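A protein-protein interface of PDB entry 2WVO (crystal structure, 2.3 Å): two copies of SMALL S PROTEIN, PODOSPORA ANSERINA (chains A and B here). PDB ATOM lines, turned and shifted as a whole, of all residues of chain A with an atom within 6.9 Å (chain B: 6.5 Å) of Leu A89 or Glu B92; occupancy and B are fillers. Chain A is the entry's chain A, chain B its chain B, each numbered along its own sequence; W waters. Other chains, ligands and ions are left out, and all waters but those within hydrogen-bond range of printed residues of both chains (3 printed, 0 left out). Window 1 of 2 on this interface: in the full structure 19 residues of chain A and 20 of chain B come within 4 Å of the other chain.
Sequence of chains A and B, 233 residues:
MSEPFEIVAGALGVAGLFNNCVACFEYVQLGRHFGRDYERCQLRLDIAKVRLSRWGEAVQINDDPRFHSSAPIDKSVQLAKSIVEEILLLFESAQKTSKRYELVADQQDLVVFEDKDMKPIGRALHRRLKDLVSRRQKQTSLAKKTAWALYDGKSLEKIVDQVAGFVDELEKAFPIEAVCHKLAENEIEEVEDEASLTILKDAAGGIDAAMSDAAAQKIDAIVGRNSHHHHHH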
ATOM      1  N   PRO A   4     -26.353 -31.042 -15.808  1.00  0.00           N
ATOM      2  CA  PRO A   4     -25.709 -29.779 -15.399  1.00  0.00           C
ATOM      3  C   PRO A   4     -25.242 -29.791 -13.943  1.00  0.00           C
ATOM      4  O   PRO A   4     -24.133 -29.345 -13.667  1.00  0.00           O
ATOM      5  CB  PRO A   4     -26.810 -28.730 -15.620  1.00  0.00           C
ATOM      6  CG  PRO A   4     -27.662 -29.310 -16.692  1.00  0.00           C
ATOM      7  CD  PRO A   4     -27.660 -30.792 -16.454  1.00  0.00           C
ATOM      8  N   PHE A   5     -26.085 -30.317 -13.046  1.00  0.00           N
ATOM      9  CA  PHE A   5     -25.773 -30.519 -11.626  1.00  0.00           C
ATOM     10  C   PHE A   5     -24.491 -31.345 -11.400  1.00  0.00           C
ATOM     11  O   PHE A   5     -23.650 -30.973 -10.583  1.00  0.00           O
ATOM     12  CB  PHE A   5     -26.973 -31.179 -10.914  1.00  0.00           C
ATOM     13  CG  PHE A   5     -26.871 -31.190  -9.405  1.00  0.00           C
ATOM     14  CD1 PHE A   5     -27.429 -30.158  -8.649  1.00  0.00           C
ATOM     15  CD2 PHE A   5     -26.212 -32.231  -8.736  1.00  0.00           C
ATOM     16  CE1 PHE A   5     -27.341 -30.162  -7.253  1.00  0.00           C
ATOM     17  CE2 PHE A   5     -26.113 -32.235  -7.342  1.00  0.00           C
ATOM     18  CZ  PHE A   5     -26.682 -31.206  -6.601  1.00  0.00           C
ATOM     19  N   VAL A   8     -21.353 -29.250 -12.366  1.00  0.00           N
ATOM     20  CA  VAL A   8     -21.050 -28.291 -11.289  1.00  0.00           C
ATOM     21  C   VAL A   8     -20.455 -28.968 -10.036  1.00  0.00           C
ATOM     22  O   VAL A   8     -19.627 -28.372  -9.333  1.00  0.00           O
ATOM     23  CB  VAL A   8     -22.290 -27.445 -10.893  1.00  0.00           C
ATOM     24  CG1 VAL A   8     -21.961 -26.481  -9.737  1.00  0.00           C
ATOM     25  CG2 VAL A   8     -22.825 -26.675 -12.096  1.00  0.00           C
ATOM     26  N   SER A  82     -18.042 -18.470 -10.964  1.00  0.00           N
ATOM     27  CA  SER A  82     -19.302 -18.418 -10.256  1.00  0.00           C
ATOM     28  C   SER A  82     -20.448 -18.241 -11.255  1.00  0.00           C
ATOM     29  O   SER A  82     -21.441 -18.962 -11.209  1.00  0.00           O
ATOM     30  CB  SER A  82     -19.259 -17.257  -9.264  1.00  0.00           C
ATOM     31  OG  SER A  82     -20.510 -17.105  -8.628  1.00  0.00           O
ATOM     32  N   VAL A  84     -20.597 -18.883 -14.524  1.00  0.00           N
ATOM     33  CA  VAL A  84     -20.713 -20.019 -15.431  1.00  0.00           C
ATOM     34  C   VAL A  84     -21.326 -21.239 -14.695  1.00  0.00           C
ATOM     35  O   VAL A  84     -22.116 -22.006 -15.259  1.00  0.00           O
ATOM     36  CB  VAL A  84     -19.303 -20.201 -16.120  1.00  0.00           C
ATOM     37  CG1 VAL A  84     -18.722 -21.553 -15.968  1.00  0.00           C
ATOM     38  CG2 VAL A  84     -19.270 -19.631 -17.561  1.00  0.00           C
ATOM     39  N   GLU A  85     -21.006 -21.378 -13.408  1.00  0.00           N
ATOM     40  CA  GLU A  85     -21.700 -22.331 -12.540  1.00  0.00           C
ATOM     41  C   GLU A  85     -23.192 -21.980 -12.384  1.00  0.00           C
ATOM     42  O   GLU A  85     -24.045 -22.870 -12.412  1.00  0.00           O
ATOM     43  CB  GLU A  85     -21.022 -22.397 -11.166  1.00  0.00           C
ATOM     44  CG  GLU A  85     -19.746 -23.196 -11.177  1.00  0.00           C
ATOM     45  CD  GLU A  85     -18.934 -23.063  -9.904  1.00  0.00           C
ATOM     46  OE1 GLU A  85     -18.026 -23.896  -9.699  1.00  0.00           O
ATOM     47  OE2 GLU A  85     -19.186 -22.136  -9.104  1.00  0.00           O
ATOM     48  N   GLU A  86     -23.495 -20.687 -12.228  1.00  0.00           N
ATOM     49  CA  GLU A  86     -24.883 -20.217 -12.131  1.00  0.00           C
ATOM     50  C   GLU A  86     -25.683 -20.493 -13.420  1.00  0.00           C
ATOM     51  O   GLU A  86     -26.842 -20.880 -13.354  1.00  0.00           O
ATOM     52  CB  GLU A  86     -24.998 -18.738 -11.611  1.00  0.00           C
ATOM     53  CG  GLU A  86     -26.207 -18.576 -10.579  1.00  0.00           C
ATOM     54  CD  GLU A  86     -26.234 -17.285  -9.763  1.00  0.00           C
ATOM     55  OE1 GLU A  86     -27.342 -16.768  -9.440  1.00  0.00           O
ATOM     56  OE2 GLU A  86     -25.174 -16.770  -9.399  1.00  0.00           O
ATOM     57  N   ILE A  87     -25.049 -20.336 -14.579  1.00  0.00           N
ATOM     58  CA  ILE A  87     -25.679 -20.667 -15.858  1.00  0.00           C
ATOM     59  C   ILE A  87     -26.060 -22.156 -15.953  1.00  0.00           C
ATOM     60  O   ILE A  87     -27.148 -22.502 -16.437  1.00  0.00           O
ATOM     61  CB  ILE A  87     -24.794 -20.257 -17.066  1.00  0.00           C
ATOM     62  CG1 ILE A  87     -24.711 -18.733 -17.175  1.00  0.00           C
ATOM     63  CG2 ILE A  87     -25.313 -20.867 -18.379  1.00  0.00           C
ATOM     64  CD1 ILE A  87     -23.671 -18.232 -18.180  1.00  0.00           C
ATOM     65  N   LEU A  88     -25.170 -23.019 -15.478  1.00  0.00           N
ATOM     66  CA  LEU A  88     -25.419 -24.455 -15.442  1.00  0.00           C
ATOM     67  C   LEU A  88     -26.586 -24.822 -14.502  1.00  0.00           C
ATOM     68  O   LEU A  88     -27.408 -25.689 -14.826  1.00  0.00           O
ATOM     69  CB  LEU A  88     -24.136 -25.166 -15.013  1.00  0.00           C
ATOM     70  CG  LEU A  88     -23.211 -26.008 -15.913  1.00  0.00           C
ATOM     71  CD1 LEU A  88     -23.583 -26.164 -17.385  1.00  0.00           C
ATOM     72  CD2 LEU A  88     -21.758 -25.607 -15.735  1.00  0.00           C
ATOM     73  N   LEU A  89     -26.639 -24.162 -13.346  1.00  0.00           N
ATOM     74  CA  LEU A  89     -27.724 -24.308 -12.372  1.00  0.00           C
ATOM     75  C   LEU A  89     -29.074 -23.878 -12.927  1.00  0.00           C
ATOM     76  O   LEU A  89     -30.118 -24.431 -12.576  1.00  0.00           O
ATOM     77  CB  LEU A  89     -27.392 -23.518 -11.104  1.00  0.00           C
ATOM     78  CG  LEU A  89     -26.817 -24.272  -9.884  1.00  0.00           C
ATOM     79  CD1 LEU A  89     -26.160 -25.612 -10.191  1.00  0.00           C
ATOM     80  CD2 LEU A  89     -25.878 -23.384  -9.091  1.00  0.00           C
ATOM     81  N   LEU A  90     -29.024 -22.897 -13.810  1.00  0.00           N
ATOM     82  CA  LEU A  90     -30.168 -22.405 -14.563  1.00  0.00           C
ATOM     83  C   LEU A  90     -30.732 -23.464 -15.522  1.00  0.00           C
ATOM     84  O   LEU A  90     -31.946 -23.636 -15.633  1.00  0.00           O
ATOM     85  CB  LEU A  90     -29.693 -21.168 -15.329  1.00  0.00           C
ATOM     86  CG  LEU A  90     -30.549 -20.166 -16.061  1.00  0.00           C
ATOM     87  CD1 LEU A  90     -31.548 -19.497 -15.091  1.00  0.00           C
ATOM     88  CD2 LEU A  90     -29.630 -19.118 -16.704  1.00  0.00           C
ATOM     89  N   PHE A  91     -29.850 -24.169 -16.221  1.00  0.00           N
ATOM     90  CA  PHE A  91     -30.267 -25.283 -17.072  1.00  0.00           C
ATOM     91  C   PHE A  91     -30.785 -26.467 -16.252  1.00  0.00           C
ATOM     92  O   PHE A  91     -31.732 -27.125 -16.646  1.00  0.00           O
ATOM     93  CB  PHE A  91     -29.116 -25.728 -17.992  1.00  0.00           C
ATOM     94  CG  PHE A  91     -28.986 -24.901 -19.247  1.00  0.00           C
ATOM     95  CD1 PHE A  91     -28.001 -23.926 -19.357  1.00  0.00           C
ATOM     96  CD2 PHE A  91     -29.858 -25.095 -20.321  1.00  0.00           C
ATOM     97  CE1 PHE A  91     -27.875 -23.163 -20.525  1.00  0.00           C
ATOM     98  CE2 PHE A  91     -29.737 -24.335 -21.482  1.00  0.00           C
ATOM     99  CZ  PHE A  91     -28.743 -23.365 -21.581  1.00  0.00           C
ATOM    100  N   GLU A  92     -30.149 -26.732 -15.117  1.00  0.00           N
ATOM    101  CA  GLU A  92     -30.564 -27.791 -14.221  1.00  0.00           C
ATOM    102  C   GLU A  92     -32.019 -27.581 -13.765  1.00  0.00           C
ATOM    103  O   GLU A  92     -32.856 -28.495 -13.820  1.00  0.00           O
ATOM    104  CB  GLU A  92     -29.610 -27.852 -13.016  1.00  0.00           C
ATOM    105  CG  GLU A  92     -30.020 -28.857 -11.906  1.00  0.00           C
ATOM    106  CD  GLU A  92     -30.036 -30.323 -12.371  1.00  0.00           C
ATOM    107  OE1 GLU A  92     -29.385 -30.654 -13.395  1.00  0.00           O
ATOM    108  OE2 GLU A  92     -30.683 -31.155 -11.684  1.00  0.00           O
ATOM    109  N   SER A  93     -32.293 -26.363 -13.318  1.00  0.00           N
ATOM    110  CA  SER A  93     -33.603 -25.963 -12.813  1.00  0.00           C
ATOM    111  C   SER A  93     -34.679 -25.930 -13.915  1.00  0.00           C
ATOM    112  O   SER A  93     -35.821 -26.316 -13.685  1.00  0.00           O
ATOM    113  CB  SER A  93     -33.455 -24.627 -12.072  1.00  0.00           C
ATOM    114  OG  SER A  93     -34.610 -23.839 -12.222  1.00  0.00           O
ATOM    115  N   ALA A  94     -34.308 -25.512 -15.121  1.00  0.00           N
ATOM    116  CA  ALA A  94     -35.212 -25.589 -16.266  1.00  0.00           C
ATOM    117  C   ALA A  94     -35.562 -27.038 -16.620  1.00  0.00           C
ATOM    118  O   ALA A  94     -36.698 -27.328 -16.965  1.00  0.00           O
ATOM    119  CB  ALA A  94     -34.613 -24.857 -17.487  1.00  0.00           C
ATOM    120  N   SER B   2     -21.933 -24.197  -2.156  1.00  0.00           N
ATOM    121  CA  SER B   2     -22.205 -24.123  -0.680  1.00  0.00           C
ATOM    122  C   SER B   2     -23.210 -25.195  -0.217  1.00  0.00           C
ATOM    123  O   SER B   2     -23.503 -26.128  -0.979  1.00  0.00           O
ATOM    124  CB  SER B   2     -22.612 -22.698  -0.252  1.00  0.00           C
ATOM    125  OG  SER B   2     -23.478 -22.083  -1.193  1.00  0.00           O
ATOM    126  N   GLU B   3     -23.705 -25.074   1.020  1.00  0.00           N
ATOM    127  CA  GLU B   3     -24.521 -26.127   1.665  1.00  0.00           C
ATOM    128  C   GLU B   3     -25.747 -26.614   0.890  1.00  0.00           C
ATOM    129  O   GLU B   3     -25.891 -27.828   0.728  1.00  0.00           O
ATOM    130  CB  GLU B   3     -24.925 -25.752   3.101  1.00  0.00           C
ATOM    131  CG  GLU B   3     -24.005 -26.294   4.166  1.00  0.00           C
ATOM    132  CD  GLU B   3     -24.413 -27.669   4.673  1.00  0.00           C
ATOM    133  OE1 GLU B   3     -24.307 -28.661   3.910  1.00  0.00           O
ATOM    134  OE2 GLU B   3     -24.825 -27.754   5.859  1.00  0.00           O
ATOM    135  N   PRO B   4     -26.640 -25.695   0.428  1.00  0.00           N
ATOM    136  CA  PRO B   4     -27.840 -26.155  -0.317  1.00  0.00           C
ATOM    137  C   PRO B   4     -27.538 -27.134  -1.466  1.00  0.00           C
ATOM    138  O   PRO B   4     -28.229 -28.143  -1.583  1.00  0.00           O
ATOM    139  CB  PRO B   4     -28.466 -24.850  -0.840  1.00  0.00           C
ATOM    140  CG  PRO B   4     -28.020 -23.808   0.135  1.00  0.00           C
ATOM    141  CD  PRO B   4     -26.631 -24.223   0.582  1.00  0.00           C
ATOM    142  N   PHE B   5     -26.518 -26.848  -2.278  1.00  0.00           N
ATOM    143  CA  PHE B   5     -26.051 -27.763  -3.337  1.00  0.00           C
ATOM    144  C   PHE B   5     -25.661 -29.150  -2.788  1.00  0.00           C
ATOM    145  O   PHE B   5     -26.009 -30.175  -3.375  1.00  0.00           O
ATOM    146  CB  PHE B   5     -24.865 -27.156  -4.094  1.00  0.00           C
ATOM    147  CG  PHE B   5     -24.433 -27.941  -5.315  1.00  0.00           C
ATOM    148  CD1 PHE B   5     -24.904 -27.597  -6.586  1.00  0.00           C
ATOM    149  CD2 PHE B   5     -23.526 -29.002  -5.203  1.00  0.00           C
ATOM    150  CE1 PHE B   5     -24.489 -28.304  -7.729  1.00  0.00           C
ATOM    151  CE2 PHE B   5     -23.112 -29.719  -6.336  1.00  0.00           C
ATOM    152  CZ  PHE B   5     -23.597 -29.369  -7.603  1.00  0.00           C
ATOM    153  N   GLU B   6     -24.931 -29.161  -1.673  1.00  0.00           N
ATOM    154  CA  GLU B   6     -24.519 -30.403  -1.010  1.00  0.00           C
ATOM    155  C   GLU B   6     -25.711 -31.184  -0.452  1.00  0.00           C
ATOM    156  O   GLU B   6     -25.741 -32.411  -0.514  1.00  0.00           O
ATOM    157  CB  GLU B   6     -23.487 -30.116   0.093  1.00  0.00           C
ATOM    158  CG  GLU B   6     -22.185 -29.455  -0.422  1.00  0.00           C
ATOM    159  CD  GLU B   6     -21.526 -30.216  -1.592  1.00  0.00           C
ATOM    160  OE1 GLU B   6     -21.492 -31.475  -1.561  1.00  0.00           O
ATOM    161  OE2 GLU B   6     -21.031 -29.553  -2.543  1.00  0.00           O
ATOM    162  N   ILE B  87     -36.155 -25.215  -4.610  1.00  0.00           N
ATOM    163  CA  ILE B  87     -36.033 -24.178  -3.585  1.00  0.00           C
ATOM    164  C   ILE B  87     -34.607 -24.114  -3.026  1.00  0.00           C
ATOM    165  O   ILE B  87     -34.040 -23.032  -2.862  1.00  0.00           O
ATOM    166  CB  ILE B  87     -37.055 -24.365  -2.434  1.00  0.00           C
ATOM    167  CG1 ILE B  87     -38.472 -24.060  -2.937  1.00  0.00           C
ATOM    168  CG2 ILE B  87     -36.680 -23.500  -1.221  1.00  0.00           C
ATOM    169  CD1 ILE B  87     -39.603 -24.584  -2.038  1.00  0.00           C
ATOM    170  N   LEU B  88     -34.023 -25.275  -2.765  1.00  0.00           N
ATOM    171  CA  LEU B  88     -32.632 -25.356  -2.348  1.00  0.00           C
ATOM    172  C   LEU B  88     -31.650 -24.780  -3.395  1.00  0.00           C
ATOM    173  O   LEU B  88     -30.686 -24.098  -3.039  1.00  0.00           O
ATOM    174  CB  LEU B  88     -32.289 -26.820  -2.043  1.00  0.00           C
ATOM    175  CG  LEU B  88     -32.195 -27.381  -0.612  1.00  0.00           C
ATOM    176  CD1 LEU B  88     -32.607 -26.439   0.503  1.00  0.00           C
ATOM    177  CD2 LEU B  88     -32.854 -28.744  -0.492  1.00  0.00           C
ATOM    178  N   LEU B  89     -31.898 -25.062  -4.674  1.00  0.00           N
ATOM    179  CA  LEU B  89     -31.091 -24.513  -5.775  1.00  0.00           C
ATOM    180  C   LEU B  89     -31.174 -22.981  -5.867  1.00  0.00           C
ATOM    181  O   LEU B  89     -30.190 -22.300  -6.187  1.00  0.00           O
ATOM    182  CB  LEU B  89     -31.509 -25.163  -7.097  1.00  0.00           C
ATOM    183  CG  LEU B  89     -30.738 -26.323  -7.770  1.00  0.00           C
ATOM    184  CD1 LEU B  89     -29.669 -27.024  -6.905  1.00  0.00           C
ATOM    185  CD2 LEU B  89     -31.720 -27.331  -8.365  1.00  0.00           C
ATOM    186  N   LEU B  90     -32.358 -22.456  -5.584  1.00  0.00           N
ATOM    187  CA  LEU B  90     -32.639 -21.021  -5.547  1.00  0.00           C
ATOM    188  C   LEU B  90     -31.837 -20.309  -4.439  1.00  0.00           C
ATOM    189  O   LEU B  90     -31.246 -19.248  -4.657  1.00  0.00           O
ATOM    190  CB  LEU B  90     -34.159 -20.854  -5.383  1.00  0.00           C
ATOM    191  CG  LEU B  90     -34.957 -19.627  -4.937  1.00  0.00           C
ATOM    192  CD1 LEU B  90     -34.945 -18.561  -6.032  1.00  0.00           C
ATOM    193  CD2 LEU B  90     -36.405 -20.042  -4.630  1.00  0.00           C
ATOM    194  N   PHE B  91     -31.804 -20.910  -3.253  1.00  0.00           N
ATOM    195  CA  PHE B  91     -30.959 -20.435  -2.168  1.00  0.00           C
ATOM    196  C   PHE B  91     -29.479 -20.528  -2.499  1.00  0.00           C
ATOM    197  O   PHE B  91     -28.713 -19.669  -2.119  1.00  0.00           O
ATOM    198  CB  PHE B  91     -31.238 -21.227  -0.888  1.00  0.00           C
ATOM    199  CG  PHE B  91     -32.342 -20.655  -0.065  1.00  0.00           C
ATOM    200  CD1 PHE B  91     -33.582 -21.283  -0.010  1.00  0.00           C
ATOM    201  CD2 PHE B  91     -32.144 -19.482   0.667  1.00  0.00           C
ATOM    202  CE1 PHE B  91     -34.619 -20.753   0.772  1.00  0.00           C
ATOM    203  CE2 PHE B  91     -33.177 -18.948   1.449  1.00  0.00           C
ATOM    204  CZ  PHE B  91     -34.415 -19.585   1.495  1.00  0.00           C
ATOM    205  N   GLU B  92     -29.082 -21.578  -3.204  1.00  0.00           N
ATOM    206  CA  GLU B  92     -27.704 -21.723  -3.612  1.00  0.00           C
ATOM    207  C   GLU B  92     -27.241 -20.667  -4.655  1.00  0.00           C
ATOM    208  O   GLU B  92     -26.138 -20.140  -4.538  1.00  0.00           O
ATOM    209  CB  GLU B  92     -27.448 -23.161  -4.073  1.00  0.00           C
ATOM    210  CG  GLU B  92     -26.168 -23.754  -3.447  1.00  0.00           C
ATOM    211  CD  GLU B  92     -25.039 -23.670  -4.401  1.00  0.00           C
ATOM    212  OE1 GLU B  92     -25.354 -23.736  -5.614  1.00  0.00           O
ATOM    213  OE2 GLU B  92     -23.864 -23.537  -3.972  1.00  0.00           O
ATOM    214  N   SER B  93     -28.079 -20.358  -5.649  1.00  0.00           N
ATOM    215  CA  SER B  93     -27.813 -19.240  -6.578  1.00  0.00           C
ATOM    216  C   SER B  93     -27.755 -17.879  -5.903  1.00  0.00           C
ATOM    217  O   SER B  93     -26.928 -17.054  -6.251  1.00  0.00           O
ATOM    218  CB  SER B  93     -28.864 -19.176  -7.681  1.00  0.00           C
ATOM    219  OG  SER B  93     -28.790 -20.362  -8.436  1.00  0.00           O
ATOM    220  N   ALA B  94     -28.666 -17.647  -4.970  1.00  0.00           N
ATOM    221  CA  ALA B  94     -28.677 -16.435  -4.170  1.00  0.00           C
ATOM    222  C   ALA B  94     -27.355 -16.262  -3.424  1.00  0.00           C
ATOM    223  O   ALA B  94     -26.819 -15.166  -3.377  1.00  0.00           O
ATOM    224  CB  ALA B  94     -29.861 -16.451  -3.201  1.00  0.00           C
ATOM    225  N   GLN B  95     -26.823 -17.345  -2.863  1.00  0.00           N
ATOM    226  CA  GLN B  95     -25.530 -17.299  -2.172  1.00  0.00           C
ATOM    227  C   GLN B  95     -24.360 -17.030  -3.120  1.00  0.00           C
ATOM    228  O   GLN B  95     -23.416 -16.341  -2.758  1.00  0.00           O
ATOM    229  CB  GLN B  95     -25.291 -18.584  -1.377  1.00  0.00           C
ATOM    230  CG  GLN B  95     -26.215 -18.720  -0.200  1.00  0.00           C
ATOM    231  CD  GLN B  95     -26.109 -20.059   0.518  1.00  0.00           C
ATOM    232  OE1 GLN B  95     -27.123 -20.641   0.906  1.00  0.00           O
ATOM    233  NE2 GLN B  95     -24.890 -20.547   0.702  1.00  0.00           N
ATOM    234  N   LYS B  96     -24.434 -17.578  -4.329  1.00  0.00           N
ATOM    235  CA  LYS B  96     -23.451 -17.314  -5.367  1.00  0.00           C
ATOM    236  C   LYS B  96     -23.451 -15.839  -5.771  1.00  0.00           C
ATOM    237  O   LYS B  96     -22.395 -15.246  -5.911  1.00  0.00           O
ATOM    238  CB  LYS B  96     -23.726 -18.162  -6.605  1.00  0.00           C
ATOM    239  CG  LYS B  96     -23.528 -19.646  -6.435  1.00  0.00           C
ATOM    240  CD  LYS B  96     -23.713 -20.292  -7.777  1.00  0.00           C
ATOM    241  CE  LYS B  96     -22.808 -21.473  -7.959  1.00  0.00           C
ATOM    242  NZ  LYS B  96     -21.388 -21.166  -7.827  1.00  0.00           N
ATOM    243  N   THR B  97     -24.638 -15.274  -5.984  1.00  0.00           N
ATOM    244  CA  THR B  97     -24.776 -13.859  -6.309  1.00  0.00           C
ATOM    245  C   THR B  97     -24.215 -12.977  -5.201  1.00  0.00           C
ATOM    246  O   THR B  97     -23.555 -11.973  -5.475  1.00  0.00           O
ATOM    247  CB  THR B  97     -26.255 -13.491  -6.562  1.00  0.00           C
ATOM    248  OG1 THR B  97     -26.714 -14.205  -7.704  1.00  0.00           O
ATOM    249  CG2 THR B  97     -26.441 -11.980  -6.808  1.00  0.00           C
ATOM    250  N   LYS B  99     -21.905 -13.858  -2.954  1.00  0.00           N
ATOM    251  CA  LYS B  99     -20.450 -14.001  -2.982  1.00  0.00           C
ATOM    252  C   LYS B  99     -19.776 -13.139  -4.053  1.00  0.00           C
ATOM    253  O   LYS B  99     -18.683 -12.588  -3.816  1.00  0.00           O
ATOM    254  CB  LYS B  99     -20.055 -15.467  -3.146  1.00  0.00           C
ATOM    255  CG  LYS B  99     -19.714 -16.140  -1.826  1.00  0.00           C
ATOM    256  CD  LYS B  99     -20.490 -17.422  -1.619  1.00  0.00           C
ATOM    257  CE  LYS B  99     -19.701 -18.678  -1.973  1.00  0.00           C
ATOM    258  NZ  LYS B  99     -20.672 -19.801  -2.225  1.00  0.00           N
HETATM  259  O   HOH W   1     -28.698 -19.951 -11.741  1.00  0.00           O
HETATM  260  O   HOH W   2     -19.998 -18.640  -6.146  1.00  0.00           O
HETATM  261  O   HOH W   3     -29.517 -15.676  -7.641  1.00  0.00           O
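Of the 17 printed residues of chain B, 6 touch a printed residue of chain A.
Hydrophobic or aromatic side chains of chain B that line the printed part of chain A: Phe B5 and Leu B89.
Of the 15 printed residues of chain A, 6 touch a printed residue of chain B.
Hydrophobic or aromatic side chains of chain A that line the printed part of chain B: Phe A5, Val A8 and Leu A89.
Along chain A the printed residues that touch a printed residue of chain B span positions 5 to 89.
Among the printed residues, 10 pairs touch across the chains.
Among the printed residues, Asp or Glu carboxylates within 4 Å of a Lys or Arg side-chain nitrogen of the other chain: Glu A85 with Lys B96.
Of the printed residues of chain B, Leu A89 touches Glu B92 (3.5 Å) and Lys B96 (3.8 Å).
Ser B2 touches none of the printed residues of chain A.
Pro B4 touches none of the printed residues of chain A.
Printed residues of chain A within 4 Å of Leu B89: Phe A5.
Of the printed residues of chain A, Glu B92 touches Leu A89 (3.5 Å).
Printed residues of chain A within 4 Å of Lys B96: Ser A82, Glu A85, Glu A86 and Leu A89.
Of the printed residues of chain A, Thr B97 touches Glu A86 (3.2 Å).
The nearest printed residue of chain B that does not touch Val A8 is Lys B96 (5.4 Å).
The side-chain carboxylate (OE2) of Glu A85 lies within salt-bridge range of the side-chain amino group (NZ) of Lys B96 (2.7 Å).
The side-chain hydroxyl of Thr B97 sits at hydrogen-bond distance from the side-chain carboxylate of Glu A86.
OE1 of Glu A86 sits close to O of Ser B93.
Water W1 lies within hydrogen-bond range of the backbone carbonyl oxygen (O) of Glu A86 (2.6 Å) and the side-chain hydroxyl (OG) of Ser B93 (3.3 Å).
Water W2 bridges the side-chain hydroxyl (OG) of Ser A82 (3.0 Å) and the side-chain amino group (NZ) of Lys B96 (3.3 Å).
Water W3 lies within hydrogen-bond range of OE1 of Glu A86 (3.0 Å), OG1 of Thr B97 (3.2 Å), O of Ser B93 (3.2 Å) and N of Ala B94 (3.4 Å).
Phe A5 touches Phe B5 (O to CZ, 3.4 Å).
Leu B89 touches Phe A5 (CD1 to CE1, 3.9 Å).
Phe B5 touches Val A8 (CE1 to CG1, 3.7 Å).
Ser A82 touches Lys B96.
Glu A86 touches Lys B96 (OE2 to CB, 3.4 Å).
CD2 of Leu A89 touches OE1 of Glu B92, at 3.5 Å.
Leu A89 touches Lys B96.
The backbone NH of Phe A5 is in hydrogen-bond range of the side-chain carboxylate of Glu A92 (3.3 Å).
The backbone NH (N) of Ser B2 lies within hydrogen-bond range of the side-chain carboxylate (OE2) of Glu B92 (2.7 Å).
OG of Ser B93 lies within hydrogen-bond range of O of Leu B89 (3.3 Å).
OG1 of Thr B97 lies within hydrogen-bond range of O of Ser B93 (3.2 Å).
Phe A5 touches its own counterpart, Phe B5.
Phe A5 touches Leu B89, but with the chains exchanged Leu A89 does not touch Phe B5 (4.01 Å).
Leu A89 touches Glu B92, but with the chains exchanged Glu A92 does not touch Leu B89 (4.2 Å).
Positions printed for both chains: 4, 5, 87, 88, 89, 90, 91, 92, 93 and 94.
Of the 10 pairs that touch across the chains among the printed residues, 1 has its exchanged pair printed and touching as well.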
